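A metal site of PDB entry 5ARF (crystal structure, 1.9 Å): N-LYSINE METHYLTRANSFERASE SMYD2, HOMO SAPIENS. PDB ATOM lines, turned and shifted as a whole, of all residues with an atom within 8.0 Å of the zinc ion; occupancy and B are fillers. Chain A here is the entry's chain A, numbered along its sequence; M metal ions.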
ATOM      1  N   HIS A  51     -11.789 -22.957  20.598  1.00  0.00           N
ATOM      2  CA  HIS A  51     -12.536 -23.266  19.359  1.00  0.00           C
ATOM      3  C   HIS A  51     -13.835 -22.436  19.316  1.00  0.00           C
ATOM      4  O   HIS A  51     -14.341 -22.064  20.366  1.00  0.00           O
ATOM      5  CB  HIS A  51     -12.881 -24.792  19.272  1.00  0.00           C
ATOM      6  CG  HIS A  51     -11.695 -25.693  19.052  1.00  0.00           C
ATOM      7  ND1 HIS A  51     -10.826 -26.045  20.063  1.00  0.00           N
ATOM      8  CD2 HIS A  51     -11.250 -26.341  17.954  1.00  0.00           C
ATOM      9  CE1 HIS A  51      -9.887 -26.856  19.603  1.00  0.00           C
ATOM     10  NE2 HIS A  51     -10.134 -27.067  18.324  1.00  0.00           N
ATOM     11  N   CYS A  52     -14.297 -22.079  18.127  1.00  0.00           N
ATOM     12  CA  CYS A  52     -15.586 -21.407  17.935  1.00  0.00           C
ATOM     13  C   CYS A  52     -16.689 -22.346  18.423  1.00  0.00           C
ATOM     14  O   CYS A  52     -16.825 -23.432  17.926  1.00  0.00           O
ATOM     15  CB  CYS A  52     -15.858 -21.074  16.443  1.00  0.00           C
ATOM     16  SG  CYS A  52     -17.312 -20.069  16.012  1.00  0.00           S
ATOM     17  N   GLU A  53     -17.492 -21.899  19.344  1.00  0.00           N
ATOM     18  CA  GLU A  53     -18.654 -22.713  19.744  1.00  0.00           C
ATOM     19  C   GLU A  53     -19.656 -23.060  18.660  1.00  0.00           C
ATOM     20  O   GLU A  53     -20.316 -24.076  18.752  1.00  0.00           O
ATOM     21  CB  GLU A  53     -19.318 -22.076  20.967  1.00  0.00           C
ATOM     22  CG  GLU A  53     -18.265 -22.119  22.061  1.00  0.00           C
ATOM     23  CD  GLU A  53     -18.817 -22.085  23.453  1.00  0.00           C
ATOM     24  OE1 GLU A  53     -19.957 -22.530  23.617  1.00  0.00           O
ATOM     25  OE2 GLU A  53     -18.055 -21.672  24.349  1.00  0.00           O
ATOM     26  N   TYR A  54     -19.702 -22.264  17.600  1.00  0.00           N
ATOM     27  CA  TYR A  54     -20.658 -22.512  16.514  1.00  0.00           C
ATOM     28  C   TYR A  54     -20.103 -23.523  15.493  1.00  0.00           C
ATOM     29  O   TYR A  54     -20.764 -24.527  15.137  1.00  0.00           O
ATOM     30  CB  TYR A  54     -21.074 -21.225  15.822  1.00  0.00           C
ATOM     31  CG  TYR A  54     -22.140 -21.513  14.782  1.00  0.00           C
ATOM     32  CD1 TYR A  54     -23.387 -22.044  15.171  1.00  0.00           C
ATOM     33  CD2 TYR A  54     -21.896 -21.338  13.439  1.00  0.00           C
ATOM     34  CE1 TYR A  54     -24.354 -22.346  14.226  1.00  0.00           C
ATOM     35  CE2 TYR A  54     -22.841 -21.619  12.493  1.00  0.00           C
ATOM     36  CZ  TYR A  54     -24.059 -22.128  12.876  1.00  0.00           C
ATOM     37  OH  TYR A  54     -24.992 -22.379  11.902  1.00  0.00           O
ATOM     38  N   CYS A  55     -18.907 -23.266  15.019  1.00  0.00           N
ATOM     39  CA  CYS A  55     -18.339 -24.063  13.940  1.00  0.00           C
ATOM     40  C   CYS A  55     -17.151 -24.932  14.277  1.00  0.00           C
ATOM     41  O   CYS A  55     -16.664 -25.653  13.422  1.00  0.00           O
ATOM     42  CB  CYS A  55     -18.013 -23.115  12.765  1.00  0.00           C
ATOM     43  SG  CYS A  55     -16.534 -22.118  13.049  1.00  0.00           S
ATOM     44  N   PHE A  56     -16.666 -24.885  15.523  1.00  0.00           N
ATOM     45  CA  PHE A  56     -15.554 -25.703  15.986  1.00  0.00           C
ATOM     46  C   PHE A  56     -14.177 -25.297  15.428  1.00  0.00           C
ATOM     47  O   PHE A  56     -13.183 -25.913  15.708  1.00  0.00           O
ATOM     48  CB  PHE A  56     -15.870 -27.230  15.837  1.00  0.00           C
ATOM     49  CG  PHE A  56     -16.839 -27.788  16.887  1.00  0.00           C
ATOM     50  CD1 PHE A  56     -17.884 -27.032  17.415  1.00  0.00           C
ATOM     51  CD2 PHE A  56     -16.732 -29.110  17.299  1.00  0.00           C
ATOM     52  CE1 PHE A  56     -18.756 -27.545  18.384  1.00  0.00           C
ATOM     53  CE2 PHE A  56     -17.663 -29.652  18.202  1.00  0.00           C
ATOM     54  CZ  PHE A  56     -18.687 -28.874  18.728  1.00  0.00           C
ATOM     55  N   THR A  57     -14.092 -24.169  14.718  1.00  0.00           N
ATOM     56  CA  THR A  57     -12.831 -23.781  14.154  1.00  0.00           C
ATOM     57  C   THR A  57     -11.972 -23.248  15.249  1.00  0.00           C
ATOM     58  O   THR A  57     -12.428 -22.431  16.047  1.00  0.00           O
ATOM     59  CB  THR A  57     -13.017 -22.692  13.113  1.00  0.00           C
ATOM     60  OG1 THR A  57     -13.836 -23.198  12.042  1.00  0.00           O
ATOM     61  CG2 THR A  57     -11.651 -22.170  12.595  1.00  0.00           C
ATOM     62  N   ARG A  58     -10.740 -23.703  15.289  1.00  0.00           N
ATOM     63  CA  ARG A  58      -9.773 -23.204  16.238  1.00  0.00           C
ATOM     64  C   ARG A  58      -9.148 -21.872  15.776  1.00  0.00           C
ATOM     65  O   ARG A  58      -8.584 -21.800  14.703  1.00  0.00           O
ATOM     66  CB  ARG A  58      -8.643 -24.207  16.442  1.00  0.00           C
ATOM     67  CG  ARG A  58      -7.663 -23.716  17.472  1.00  0.00           C
ATOM     68  CD  ARG A  58      -7.297 -24.757  18.526  1.00  0.00           C
ATOM     69  NE  ARG A  58      -5.874 -24.647  18.705  1.00  0.00           N
ATOM     70  CZ  ARG A  58      -4.995 -25.095  17.817  1.00  0.00           C
ATOM     71  NH1 ARG A  58      -5.430 -25.743  16.725  1.00  0.00           N
ATOM     72  NH2 ARG A  58      -3.691 -24.936  18.015  1.00  0.00           N
ATOM     73  N   LYS A  59      -9.176 -20.883  16.654  1.00  0.00           N
ATOM     74  CA  LYS A  59      -8.552 -19.606  16.381  1.00  0.00           C
ATOM     75  C   LYS A  59      -7.921 -19.074  17.642  1.00  0.00           C
ATOM     76  O   LYS A  59      -8.474 -19.259  18.741  1.00  0.00           O
ATOM     77  CB  LYS A  59      -9.600 -18.605  15.903  1.00  0.00           C
ATOM     78  CG  LYS A  59     -10.248 -18.971  14.583  1.00  0.00           C
ATOM     79  CD  LYS A  59     -11.457 -18.123  14.247  1.00  0.00           C
ATOM     80  CE  LYS A  59     -11.180 -16.705  13.860  1.00  0.00           C
ATOM     81  NZ  LYS A  59     -10.567 -16.728  12.516  1.00  0.00           N
ATOM     82  N   LEU A  62     -10.680 -15.147  19.642  1.00  0.00           N
ATOM     83  CA  LEU A  62     -12.066 -15.438  19.313  1.00  0.00           C
ATOM     84  C   LEU A  62     -12.773 -14.271  19.862  1.00  0.00           C
ATOM     85  O   LEU A  62     -12.226 -13.618  20.752  1.00  0.00           O
ATOM     86  CB  LEU A  62     -12.509 -16.717  20.006  1.00  0.00           C
ATOM     87  CG  LEU A  62     -12.358 -18.116  19.364  1.00  0.00           C
ATOM     88  CD1 LEU A  62     -12.354 -18.109  17.825  1.00  0.00           C
ATOM     89  CD2 LEU A  62     -11.232 -18.913  19.983  1.00  0.00           C
ATOM     90  N   PHE A  72     -17.222 -18.152  22.968  1.00  0.00           N
ATOM     91  CA  PHE A  72     -16.264 -17.616  22.050  1.00  0.00           C
ATOM     92  C   PHE A  72     -16.606 -18.070  20.669  1.00  0.00           C
ATOM     93  O   PHE A  72     -17.028 -19.230  20.481  1.00  0.00           O
ATOM     94  CB  PHE A  72     -14.885 -18.152  22.434  1.00  0.00           C
ATOM     95  CG  PHE A  72     -14.391 -17.643  23.760  1.00  0.00           C
ATOM     96  CD1 PHE A  72     -14.868 -18.190  24.944  1.00  0.00           C
ATOM     97  CD2 PHE A  72     -13.456 -16.611  23.818  1.00  0.00           C
ATOM     98  CE1 PHE A  72     -14.419 -17.715  26.171  1.00  0.00           C
ATOM     99  CE2 PHE A  72     -13.013 -16.105  25.042  1.00  0.00           C
ATOM    100  CZ  PHE A  72     -13.496 -16.671  26.215  1.00  0.00           C
ATOM    101  N   TYR A  73     -16.389 -17.173  19.723  1.00  0.00           N
ATOM    102  CA  TYR A  73     -16.838 -17.302  18.344  1.00  0.00           C
ATOM    103  C   TYR A  73     -15.864 -16.699  17.343  1.00  0.00           C
ATOM    104  O   TYR A  73     -15.116 -15.791  17.679  1.00  0.00           O
ATOM    105  CB  TYR A  73     -18.188 -16.611  18.209  1.00  0.00           C
ATOM    106  CG  TYR A  73     -19.269 -17.228  19.084  1.00  0.00           C
ATOM    107  CD1 TYR A  73     -19.846 -18.430  18.751  1.00  0.00           C
ATOM    108  CD2 TYR A  73     -19.694 -16.583  20.240  1.00  0.00           C
ATOM    109  CE1 TYR A  73     -20.834 -18.994  19.542  1.00  0.00           C
ATOM    110  CE2 TYR A  73     -20.659 -17.117  21.050  1.00  0.00           C
ATOM    111  CZ  TYR A  73     -21.264 -18.335  20.678  1.00  0.00           C
ATOM    112  OH  TYR A  73     -22.258 -18.873  21.483  1.00  0.00           O
ATOM    113  N   CYS A  74     -15.862 -17.231  16.117  1.00  0.00           N
ATOM    114  CA  CYS A  74     -15.046 -16.704  15.010  1.00  0.00           C
ATOM    115  C   CYS A  74     -15.296 -15.235  14.719  1.00  0.00           C
ATOM    116  O   CYS A  74     -14.379 -14.555  14.338  1.00  0.00           O
ATOM    117  CB  CYS A  74     -15.419 -17.425  13.720  1.00  0.00           C
ATOM    118  SG  CYS A  74     -14.898 -19.124  13.559  1.00  0.00           S
ATOM    119  N   ASN A  75     -16.553 -14.815  14.856  1.00  0.00           N
ATOM    120  CA  ASN A  75     -17.119 -13.564  14.358  1.00  0.00           C
ATOM    121  C   ASN A  75     -18.593 -13.480  14.647  1.00  0.00           C
ATOM    122  O   ASN A  75     -19.227 -14.465  15.060  1.00  0.00           O
ATOM    123  CB  ASN A  75     -16.979 -13.451  12.851  1.00  0.00           C
ATOM    124  CG  ASN A  75     -17.502 -14.650  12.108  1.00  0.00           C
ATOM    125  OD1 ASN A  75     -18.630 -15.154  12.344  1.00  0.00           O
ATOM    126  ND2 ASN A  75     -16.681 -15.154  11.200  1.00  0.00           N
ATOM    127  N   GLU A  77     -21.253 -13.527  12.918  1.00  0.00           N
ATOM    128  CA  GLU A  77     -22.184 -14.467  12.285  1.00  0.00           C
ATOM    129  C   GLU A  77     -22.209 -15.778  13.024  1.00  0.00           C
ATOM    130  O   GLU A  77     -23.279 -16.332  13.243  1.00  0.00           O
ATOM    131  CB  GLU A  77     -21.838 -14.786  10.836  1.00  0.00           C
ATOM    132  CG  GLU A  77     -22.065 -13.641   9.867  1.00  0.00           C
ATOM    133  CD  GLU A  77     -22.204 -14.113   8.417  1.00  0.00           C
ATOM    134  OE1 GLU A  77     -23.285 -14.669   8.107  1.00  0.00           O
ATOM    135  OE2 GLU A  77     -21.236 -13.934   7.612  1.00  0.00           O
ATOM    136  N   CYS A  78     -21.029 -16.300  13.366  1.00  0.00           N
ATOM    137  CA  CYS A  78     -20.918 -17.559  14.144  1.00  0.00           C
ATOM    138  C   CYS A  78     -21.694 -17.429  15.441  1.00  0.00           C
ATOM    139  O   CYS A  78     -22.528 -18.286  15.749  1.00  0.00           O
ATOM    140  CB  CYS A  78     -19.470 -17.935  14.415  1.00  0.00           C
ATOM    141  SG  CYS A  78     -18.646 -18.898  13.127  1.00  0.00           S
ATOM    142  N   GLN A  79     -21.428 -16.333  16.176  1.00  0.00           N
ATOM    143  CA  GLN A  79     -22.167 -15.984  17.397  1.00  0.00           C
ATOM    144  C   GLN A  79     -23.662 -15.881  17.163  1.00  0.00           C
ATOM    145  O   GLN A  79     -24.429 -16.578  17.870  1.00  0.00           O
ATOM    146  CB  GLN A  79     -21.651 -14.711  18.011  1.00  0.00           C
ATOM    147  CG  GLN A  79     -22.293 -14.277  19.343  1.00  0.00           C
ATOM    148  CD  GLN A  79     -21.837 -12.848  19.741  1.00  0.00           C
ATOM    149  OE1 GLN A  79     -22.037 -12.396  20.891  1.00  0.00           O
ATOM    150  NE2 GLN A  79     -21.250 -12.136  18.799  1.00  0.00           N
ATOM    151  N   GLU A  81     -25.430 -17.239  14.902  1.00  0.00           N
ATOM    152  CA  GLU A  81     -25.913 -18.569  14.552  1.00  0.00           C
ATOM    153  C   GLU A  81     -26.111 -19.524  15.745  1.00  0.00           C
ATOM    154  O   GLU A  81     -26.979 -20.427  15.734  1.00  0.00           O
ATOM    155  CB  GLU A  81     -24.954 -19.193  13.537  1.00  0.00           C
ATOM    156  CG  GLU A  81     -25.028 -18.600  12.136  1.00  0.00           C
ATOM    157  CD  GLU A  81     -26.448 -18.634  11.642  1.00  0.00           C
ATOM    158  OE1 GLU A  81     -27.077 -19.719  11.761  1.00  0.00           O
ATOM    159  OE2 GLU A  81     -26.962 -17.570  11.263  1.00  0.00           O
HETATM  160 ZN    ZN M   1     -17.058 -20.176  13.599  1.00  0.00          ZN
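The nearest printed residue that does not touch the zinc ion is Thr 57 (4.7 Å).
The side-chain sulfur (SG) of Cys 55 lies close to the side-chain hydroxyl (OG1) of Thr 57 (3.1 Å).
The backbone NH (N) of Cys 78 is in hydrogen-bond range of the side-chain amide oxygen (OD1) of Asn 75.
N of Cys 52 sits at hydrogen-bond distance from O of Thr 57 (2.8 Å).
The side-chain sulfur of Cys 52 lies close to the backbone NH of Tyr 54 (3.6 Å).
The zinc ion is bound by the side-chain sulfur (SG) of Cys 55 (2.1 Å).
The zinc ion is bound by the side-chain sulfur (SG) of Cys 78 (2.1 Å).
SG of Cys 74 binds the zinc ion (2.4 Å).
The zinc ion is bound by the side-chain sulfur (SG) of Cys 52 (2.4 Å).
The zinc ion has four donor atoms within binding distance.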
